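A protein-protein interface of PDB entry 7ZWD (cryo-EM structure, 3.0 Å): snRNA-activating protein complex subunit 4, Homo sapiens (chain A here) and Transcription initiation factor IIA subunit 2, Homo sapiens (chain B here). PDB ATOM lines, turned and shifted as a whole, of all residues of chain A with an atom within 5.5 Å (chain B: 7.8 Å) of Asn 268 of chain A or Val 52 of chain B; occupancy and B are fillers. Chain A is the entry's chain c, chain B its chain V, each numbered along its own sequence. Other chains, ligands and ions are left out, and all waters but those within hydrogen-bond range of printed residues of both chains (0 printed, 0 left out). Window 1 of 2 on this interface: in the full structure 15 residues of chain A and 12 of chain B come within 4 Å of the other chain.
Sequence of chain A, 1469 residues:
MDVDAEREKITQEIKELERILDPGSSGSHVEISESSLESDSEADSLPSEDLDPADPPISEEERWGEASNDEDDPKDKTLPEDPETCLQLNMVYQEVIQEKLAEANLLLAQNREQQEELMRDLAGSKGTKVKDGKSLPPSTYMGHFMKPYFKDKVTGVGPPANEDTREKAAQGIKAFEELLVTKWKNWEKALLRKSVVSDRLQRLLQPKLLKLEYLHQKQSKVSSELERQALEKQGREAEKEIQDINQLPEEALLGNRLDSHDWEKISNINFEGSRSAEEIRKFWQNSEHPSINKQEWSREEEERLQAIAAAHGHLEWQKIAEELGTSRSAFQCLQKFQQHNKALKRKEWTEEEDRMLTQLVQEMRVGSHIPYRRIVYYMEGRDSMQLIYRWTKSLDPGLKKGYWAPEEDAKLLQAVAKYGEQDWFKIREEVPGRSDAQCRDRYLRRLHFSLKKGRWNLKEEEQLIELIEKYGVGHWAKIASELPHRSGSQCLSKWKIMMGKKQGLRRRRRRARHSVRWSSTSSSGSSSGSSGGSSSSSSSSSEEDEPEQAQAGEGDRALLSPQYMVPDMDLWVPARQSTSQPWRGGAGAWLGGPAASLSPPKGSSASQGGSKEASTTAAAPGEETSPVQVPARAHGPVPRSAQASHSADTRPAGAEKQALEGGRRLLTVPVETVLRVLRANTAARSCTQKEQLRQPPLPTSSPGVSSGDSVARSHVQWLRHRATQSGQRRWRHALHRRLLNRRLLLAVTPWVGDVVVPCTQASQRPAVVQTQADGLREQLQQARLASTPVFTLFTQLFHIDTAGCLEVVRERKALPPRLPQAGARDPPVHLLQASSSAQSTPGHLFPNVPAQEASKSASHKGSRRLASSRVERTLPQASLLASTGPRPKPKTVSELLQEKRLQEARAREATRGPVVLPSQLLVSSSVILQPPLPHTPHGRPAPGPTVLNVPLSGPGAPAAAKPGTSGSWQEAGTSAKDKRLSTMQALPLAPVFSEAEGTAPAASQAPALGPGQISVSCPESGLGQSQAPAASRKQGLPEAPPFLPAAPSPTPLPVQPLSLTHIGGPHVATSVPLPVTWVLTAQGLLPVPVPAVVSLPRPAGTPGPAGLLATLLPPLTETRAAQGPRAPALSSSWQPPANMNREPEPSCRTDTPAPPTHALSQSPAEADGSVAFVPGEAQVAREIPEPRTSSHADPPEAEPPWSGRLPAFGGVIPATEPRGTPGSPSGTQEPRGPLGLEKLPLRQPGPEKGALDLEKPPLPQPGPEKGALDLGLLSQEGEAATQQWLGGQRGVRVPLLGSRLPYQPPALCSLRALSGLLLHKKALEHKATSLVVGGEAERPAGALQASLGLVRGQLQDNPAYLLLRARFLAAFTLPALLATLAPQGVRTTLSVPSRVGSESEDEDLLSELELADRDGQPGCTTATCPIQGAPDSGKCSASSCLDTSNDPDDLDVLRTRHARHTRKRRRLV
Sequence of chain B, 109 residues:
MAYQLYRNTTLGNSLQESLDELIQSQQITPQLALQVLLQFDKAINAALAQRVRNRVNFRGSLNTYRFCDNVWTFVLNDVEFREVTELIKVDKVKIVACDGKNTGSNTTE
OE1 of Gln 50 of chain B lies close to NZ of Lys 265 of chain A (3.4 Å).
The backbone carbonyl oxygen (O) of Gln 50 of chain B sits at hydrogen-bond distance from the side-chain amide nitrogen (ND2) of Asn 268 of chain A, 2.8 Å away.
The guanidinium group (NE) of Arg 51 of chain B is in salt-bridge range of the side-chain carboxylate (OE1) of Glu 264 of chain A.
The guanidinium group (NE) of Arg 53 of chain B is in hydrogen-bond range of the side-chain amide oxygen (OD1) of Asn 268 of chain A (3.0 Å).
Among the printed residues, merely in contact across the chains: Ile 269 of chain A with Gln 50 of chain B, Glu 264 of chain A with Gln 50 of chain B, Asn 268 of chain A with Val 52 of chain B, Asn 268 of chain A with Arg 51 of chain B and Lys 265 of chain A with Arg 51 of chain B.
Of the 11 printed residues of chain B, 4 touch a printed residue of chain A.
Along chain B the printed residues that touch a printed residue of chain A span positions 50 to 53.
Hydrophobic or aromatic side chains of chain A within 4 Å of the printed part of chain B: Ile 269.
Along chain A the printed residues that touch a printed residue of chain B span positions 264 to 269.
The backbone carbonyl oxygen (O) of Ala 46 of chain B lies close to the side-chain amide oxygen (OE1) of Gln 50 of chain B (3.5 Å).
The backbone carbonyl oxygen (O) of Glu 264 of chain A lies within hydrogen-bond range of the side-chain amide nitrogen (ND2) of Asn 268 of chain A.
Of the printed residues of chain B, Lys 265 of chain A touches Gln 50 and Arg 51.
Of chain B, only Gln 50 (2.8 Å), Arg 51 (3.8 Å), Val 52 (3.7 Å) and Arg 53 (3.0 Å) come within 4 Å of Asn 268 of chain A.
Ala 49 of chain B touches none of the printed residues of chain A.
Of the printed residues of chain A, Arg 51 of chain B touches Glu 264 (3.5 Å), Lys 265 (3.8 Å) and Asn 268 (3.8 Å).
Of chain A, only Asn 268 (3.7 Å) comes within 4 Å of Val 52 of chain B.
Of the printed residues of chain A, Arg 53 of chain B touches Asn 268 (3.0 Å).
The nearest printed residue of chain A that does not touch Val 52 of chain B is Glu 264 of chain A (5.5 Å).
The nearest printed residue of chain B that does not touch Glu 264 of chain A is Val 52 of chain B (5.5 Å).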
ATOM      1  N   GLU A 264     -24.202 -34.767  13.510  1.00  0.00           N
ATOM      2  CA  GLU A 264     -24.490 -33.567  12.740  1.00  0.00           C
ATOM      3  C   GLU A 264     -23.883 -32.349  13.412  1.00  0.00           C
ATOM      4  O   GLU A 264     -23.538 -31.368  12.749  1.00  0.00           O
ATOM      5  CB  GLU A 264     -25.995 -33.394  12.570  1.00  0.00           C
ATOM      6  CG  GLU A 264     -26.758 -34.692  12.394  1.00  0.00           C
ATOM      7  CD  GLU A 264     -27.375 -35.190  13.689  1.00  0.00           C
ATOM      8  OE1 GLU A 264     -26.712 -35.091  14.740  1.00  0.00           O
ATOM      9  OE2 GLU A 264     -28.523 -35.679  13.658  1.00  0.00           O
ATOM     10  N   LYS A 265     -23.736 -32.401  14.734  1.00  0.00           N
ATOM     11  CA  LYS A 265     -23.201 -31.261  15.465  1.00  0.00           C
ATOM     12  C   LYS A 265     -21.697 -31.152  15.287  1.00  0.00           C
ATOM     13  O   LYS A 265     -21.170 -30.059  15.061  1.00  0.00           O
ATOM     14  CB  LYS A 265     -23.551 -31.393  16.940  1.00  0.00           C
ATOM     15  CG  LYS A 265     -23.195 -30.204  17.786  1.00  0.00           C
ATOM     16  CD  LYS A 265     -23.496 -30.524  19.224  1.00  0.00           C
ATOM     17  CE  LYS A 265     -24.997 -30.654  19.439  1.00  0.00           C
ATOM     18  NZ  LYS A 265     -25.346 -30.863  20.877  1.00  0.00           N
ATOM     19  N   ILE A 266     -20.991 -32.277  15.392  1.00  0.00           N
ATOM     20  CA  ILE A 266     -19.545 -32.269  15.221  1.00  0.00           C
ATOM     21  C   ILE A 266     -19.174 -31.814  13.823  1.00  0.00           C
ATOM     22  O   ILE A 266     -18.109 -31.226  13.614  1.00  0.00           O
ATOM     23  CB  ILE A 266     -18.983 -33.666  15.528  1.00  0.00           C
ATOM     24  CG1 ILE A 266     -19.622 -34.214  16.798  1.00  0.00           C
ATOM     25  CG2 ILE A 266     -17.487 -33.621  15.666  1.00  0.00           C
ATOM     26  CD1 ILE A 266     -19.150 -35.583  17.153  1.00  0.00           C
ATOM     27  N   SER A 267     -20.041 -32.062  12.845  1.00  0.00           N
ATOM     28  CA  SER A 267     -19.746 -31.659  11.480  1.00  0.00           C
ATOM     29  C   SER A 267     -19.896 -30.165  11.271  1.00  0.00           C
ATOM     30  O   SER A 267     -19.404 -29.642  10.270  1.00  0.00           O
ATOM     31  CB  SER A 267     -20.655 -32.390  10.504  1.00  0.00           C
ATOM     32  OG  SER A 267     -20.587 -33.786  10.703  1.00  0.00           O
ATOM     33  N   ASN A 268     -20.571 -29.474  12.168  1.00  0.00           N
ATOM     34  CA  ASN A 268     -20.774 -28.042  12.019  1.00  0.00           C
ATOM     35  C   ASN A 268     -20.023 -27.227  13.050  1.00  0.00           C
ATOM     36  O   ASN A 268     -19.403 -26.222  12.703  1.00  0.00           O
ATOM     37  CB  ASN A 268     -22.268 -27.728  12.053  1.00  0.00           C
ATOM     38  CG  ASN A 268     -23.031 -28.472  11.000  1.00  0.00           C
ATOM     39  OD1 ASN A 268     -22.579 -28.610   9.869  1.00  0.00           O
ATOM     40  ND2 ASN A 268     -24.205 -28.955  11.363  1.00  0.00           N
ATOM     41  N   ILE A 269     -20.054 -27.639  14.309  1.00  0.00           N
ATOM     42  CA  ILE A 269     -19.399 -26.882  15.363  1.00  0.00           C
ATOM     43  C   ILE A 269     -17.909 -27.165  15.402  1.00  0.00           C
ATOM     44  O   ILE A 269     -17.090 -26.274  15.174  1.00  0.00           O
ATOM     45  CB  ILE A 269     -20.067 -27.193  16.716  1.00  0.00           C
ATOM     46  CG1 ILE A 269     -21.534 -26.781  16.676  1.00  0.00           C
ATOM     47  CG2 ILE A 269     -19.348 -26.487  17.836  1.00  0.00           C
ATOM     48  CD1 ILE A 269     -21.756 -25.423  16.072  1.00  0.00           C
ATOM     49  N   ASN A 270     -17.534 -28.412  15.662  1.00  0.00           N
ATOM     50  CA  ASN A 270     -16.123 -28.747  15.799  1.00  0.00           C
ATOM     51  C   ASN A 270     -15.408 -28.667  14.459  1.00  0.00           C
ATOM     52  O   ASN A 270     -14.490 -27.863  14.281  1.00  0.00           O
ATOM     53  CB  ASN A 270     -15.966 -30.125  16.422  1.00  0.00           C
ATOM     54  CG  ASN A 270     -16.617 -30.210  17.775  1.00  0.00           C
ATOM     55  OD1 ASN A 270     -15.979 -29.985  18.798  1.00  0.00           O
ATOM     56  ND2 ASN A 270     -17.898 -30.542  17.790  1.00  0.00           N
ATOM     57  N   PHE A 271     -15.814 -29.494  13.506  1.00  0.00           N
ATOM     58  CA  PHE A 271     -15.398 -29.296  12.130  1.00  0.00           C
ATOM     59  C   PHE A 271     -16.267 -28.214  11.518  1.00  0.00           C
ATOM     60  O   PHE A 271     -17.488 -28.218  11.677  1.00  0.00           O
ATOM     61  CB  PHE A 271     -15.518 -30.588  11.330  1.00  0.00           C
ATOM     62  CG  PHE A 271     -14.759 -31.735  11.915  1.00  0.00           C
ATOM     63  CD1 PHE A 271     -15.327 -32.538  12.875  1.00  0.00           C
ATOM     64  CD2 PHE A 271     -13.478 -32.011  11.501  1.00  0.00           C
ATOM     65  CE1 PHE A 271     -14.634 -33.591  13.411  1.00  0.00           C
ATOM     66  CE2 PHE A 271     -12.783 -33.063  12.036  1.00  0.00           C
ATOM     67  CZ  PHE A 271     -13.362 -33.853  12.991  1.00  0.00           C
ATOM     68  N   GLU A 272     -15.641 -27.282  10.821  1.00  0.00           N
ATOM     69  CA  GLU A 272     -16.355 -26.120  10.317  1.00  0.00           C
ATOM     70  C   GLU A 272     -17.279 -26.454   9.156  1.00  0.00           C
ATOM     71  O   GLU A 272     -17.792 -25.537   8.509  1.00  0.00           O
ATOM     72  CB  GLU A 272     -15.368 -25.025   9.894  1.00  0.00           C
ATOM     73  CG  GLU A 272     -14.318 -24.632  10.939  1.00  0.00           C
ATOM     74  CD  GLU A 272     -13.263 -25.699  11.173  1.00  0.00           C
ATOM     75  OE1 GLU A 272     -12.589 -25.655  12.225  1.00  0.00           O
ATOM     76  OE2 GLU A 272     -13.114 -26.587  10.308  1.00  0.00           O
ATOM     77  N   GLY A 273     -17.502 -27.734   8.880  1.00  0.00           N
ATOM     78  CA  GLY A 273     -18.297 -28.145   7.744  1.00  0.00           C
ATOM     79  C   GLY A 273     -17.454 -28.898   6.740  1.00  0.00           C
ATOM     80  O   GLY A 273     -17.933 -29.291   5.675  1.00  0.00           O
ATOM     81  N   ILE B  44     -34.604 -27.151  20.654  1.00  0.00           N
ATOM     82  CA  ILE B  44     -34.738 -26.821  19.244  1.00  0.00           C
ATOM     83  C   ILE B  44     -33.837 -25.660  18.883  1.00  0.00           C
ATOM     84  O   ILE B  44     -33.324 -25.599  17.762  1.00  0.00           O
ATOM     85  CB  ILE B  44     -36.198 -26.533  18.867  1.00  0.00           C
ATOM     86  CG1 ILE B  44     -36.356 -26.616  17.359  1.00  0.00           C
ATOM     87  CG2 ILE B  44     -36.610 -25.163  19.315  1.00  0.00           C
ATOM     88  CD1 ILE B  44     -37.777 -26.665  16.921  1.00  0.00           C
ATOM     89  N   ALA B  46     -30.835 -25.188  20.226  1.00  0.00           N
ATOM     90  CA  ALA B  46     -29.524 -25.814  20.098  1.00  0.00           C
ATOM     91  C   ALA B  46     -29.422 -26.627  18.815  1.00  0.00           C
ATOM     92  O   ALA B  46     -28.379 -26.627  18.151  1.00  0.00           O
ATOM     93  CB  ALA B  46     -29.242 -26.695  21.311  1.00  0.00           C
ATOM     94  N   ALA B  47     -30.497 -27.320  18.446  1.00  0.00           N
ATOM     95  CA  ALA B  47     -30.489 -28.110  17.222  1.00  0.00           C
ATOM     96  C   ALA B  47     -30.339 -27.219  16.003  1.00  0.00           C
ATOM     97  O   ALA B  47     -29.386 -27.360  15.232  1.00  0.00           O
ATOM     98  CB  ALA B  47     -31.766 -28.937  17.123  1.00  0.00           C
ATOM     99  N   LEU B  48     -31.265 -26.279  15.821  1.00  0.00           N
ATOM    100  CA  LEU B  48     -31.202 -25.399  14.664  1.00  0.00           C
ATOM    101  C   LEU B  48     -29.918 -24.591  14.618  1.00  0.00           C
ATOM    102  O   LEU B  48     -29.527 -24.141  13.540  1.00  0.00           O
ATOM    103  CB  LEU B  48     -32.398 -24.461  14.658  1.00  0.00           C
ATOM    104  CG  LEU B  48     -33.735 -25.132  14.395  1.00  0.00           C
ATOM    105  CD1 LEU B  48     -34.844 -24.290  14.948  1.00  0.00           C
ATOM    106  CD2 LEU B  48     -33.914 -25.323  12.923  1.00  0.00           C
ATOM    107  N   ALA B  49     -29.251 -24.391  15.752  1.00  0.00           N
ATOM    108  CA  ALA B  49     -27.983 -23.679  15.706  1.00  0.00           C
ATOM    109  C   ALA B  49     -26.831 -24.592  15.337  1.00  0.00           C
ATOM    110  O   ALA B  49     -25.914 -24.167  14.630  1.00  0.00           O
ATOM    111  CB  ALA B  49     -27.705 -23.011  17.050  1.00  0.00           C
ATOM    112  N   GLN B  50     -26.861 -25.839  15.783  1.00  0.00           N
ATOM    113  CA  GLN B  50     -25.713 -26.719  15.658  1.00  0.00           C
ATOM    114  C   GLN B  50     -25.907 -27.853  14.670  1.00  0.00           C
ATOM    115  O   GLN B  50     -24.974 -28.193  13.949  1.00  0.00           O
ATOM    116  CB  GLN B  50     -25.363 -27.287  17.031  1.00  0.00           C
ATOM    117  CG  GLN B  50     -24.884 -26.223  17.981  1.00  0.00           C
ATOM    118  CD  GLN B  50     -24.831 -26.702  19.411  1.00  0.00           C
ATOM    119  OE1 GLN B  50     -25.496 -27.666  19.777  1.00  0.00           O
ATOM    120  NE2 GLN B  50     -24.036 -26.027  20.231  1.00  0.00           N
ATOM    121  N   ARG B  51     -27.093 -28.448  14.603  1.00  0.00           N
ATOM    122  CA  ARG B  51     -27.315 -29.608  13.752  1.00  0.00           C
ATOM    123  C   ARG B  51     -27.880 -29.241  12.391  1.00  0.00           C
ATOM    124  O   ARG B  51     -28.453 -30.099  11.716  1.00  0.00           O
ATOM    125  CB  ARG B  51     -28.244 -30.603  14.438  1.00  0.00           C
ATOM    126  CG  ARG B  51     -27.699 -31.152  15.718  1.00  0.00           C
ATOM    127  CD  ARG B  51     -28.436 -32.397  16.119  1.00  0.00           C
ATOM    128  NE  ARG B  51     -28.179 -32.713  17.512  1.00  0.00           N
ATOM    129  CZ  ARG B  51     -28.904 -32.242  18.516  1.00  0.00           C
ATOM    130  NH1 ARG B  51     -29.934 -31.448  18.272  1.00  0.00           N
ATOM    131  NH2 ARG B  51     -28.607 -32.572  19.763  1.00  0.00           N
ATOM    132  N   VAL B  52     -27.746 -27.992  11.971  1.00  0.00           N
ATOM    133  CA  VAL B  52     -28.313 -27.543  10.709  1.00  0.00           C
ATOM    134  C   VAL B  52     -27.304 -26.656  10.009  1.00  0.00           C
ATOM    135  O   VAL B  52     -26.826 -25.677  10.589  1.00  0.00           O
ATOM    136  CB  VAL B  52     -29.636 -26.788  10.909  1.00  0.00           C
ATOM    137  CG1 VAL B  52     -30.025 -26.093   9.636  1.00  0.00           C
ATOM    138  CG2 VAL B  52     -30.717 -27.746  11.322  1.00  0.00           C
ATOM    139  N   ARG B  53     -26.984 -26.994   8.767  1.00  0.00           N
ATOM    140  CA  ARG B  53     -26.138 -26.141   7.945  1.00  0.00           C
ATOM    141  C   ARG B  53     -26.597 -26.269   6.507  1.00  0.00           C
ATOM    142  O   ARG B  53     -26.154 -27.173   5.795  1.00  0.00           O
ATOM    143  CB  ARG B  53     -24.667 -26.520   8.071  1.00  0.00           C
ATOM    144  CG  ARG B  53     -23.728 -25.470   7.511  1.00  0.00           C
ATOM    145  CD  ARG B  53     -22.316 -26.003   7.369  1.00  0.00           C
ATOM    146  NE  ARG B  53     -22.295 -27.435   7.095  1.00  0.00           N
ATOM    147  CZ  ARG B  53     -22.047 -27.965   5.901  1.00  0.00           C
ATOM    148  NH1 ARG B  53     -21.798 -27.179   4.864  1.00  0.00           N
ATOM    149  NH2 ARG B  53     -22.048 -29.282   5.748  1.00  0.00           N
ATOM    150  N   ASN B  54     -27.484 -25.375   6.091  1.00  0.00           N
ATOM    151  CA  ASN B  54     -27.866 -25.260   4.696  1.00  0.00           C
ATOM    152  C   ASN B  54     -28.451 -23.875   4.496  1.00  0.00           C
ATOM    153  O   ASN B  54     -29.313 -23.432   5.254  1.00  0.00           O
ATOM    154  CB  ASN B  54     -28.859 -26.345   4.278  1.00  0.00           C
ATOM    155  CG  ASN B  54     -30.239 -26.110   4.819  1.00  0.00           C
ATOM    156  OD1 ASN B  54     -31.070 -25.477   4.176  1.00  0.00           O
ATOM    157  ND2 ASN B  54     -30.496 -26.622   6.006  1.00  0.00           N
ATOM    158  N   ARG B  55     -27.959 -23.192   3.474  1.00  0.00           N
ATOM    159  CA  ARG B  55     -28.327 -21.815   3.214  1.00  0.00           C
ATOM    160  C   ARG B  55     -29.361 -21.762   2.107  1.00  0.00           C
ATOM    161  O   ARG B  55     -29.193 -22.393   1.062  1.00  0.00           O
ATOM    162  CB  ARG B  55     -27.109 -20.990   2.819  1.00  0.00           C
ATOM    163  CG  ARG B  55     -27.388 -19.510   2.765  1.00  0.00           C
ATOM    164  CD  ARG B  55     -26.178 -18.722   2.317  1.00  0.00           C
ATOM    165  NE  ARG B  55     -26.038 -18.732   0.867  1.00  0.00           N
ATOM    166  CZ  ARG B  55     -25.467 -17.758   0.168  1.00  0.00           C
ATOM    167  NH1 ARG B  55     -24.982 -16.694   0.787  1.00  0.00           N
ATOM    168  NH2 ARG B  55     -25.383 -17.848  -1.151  1.00  0.00           N
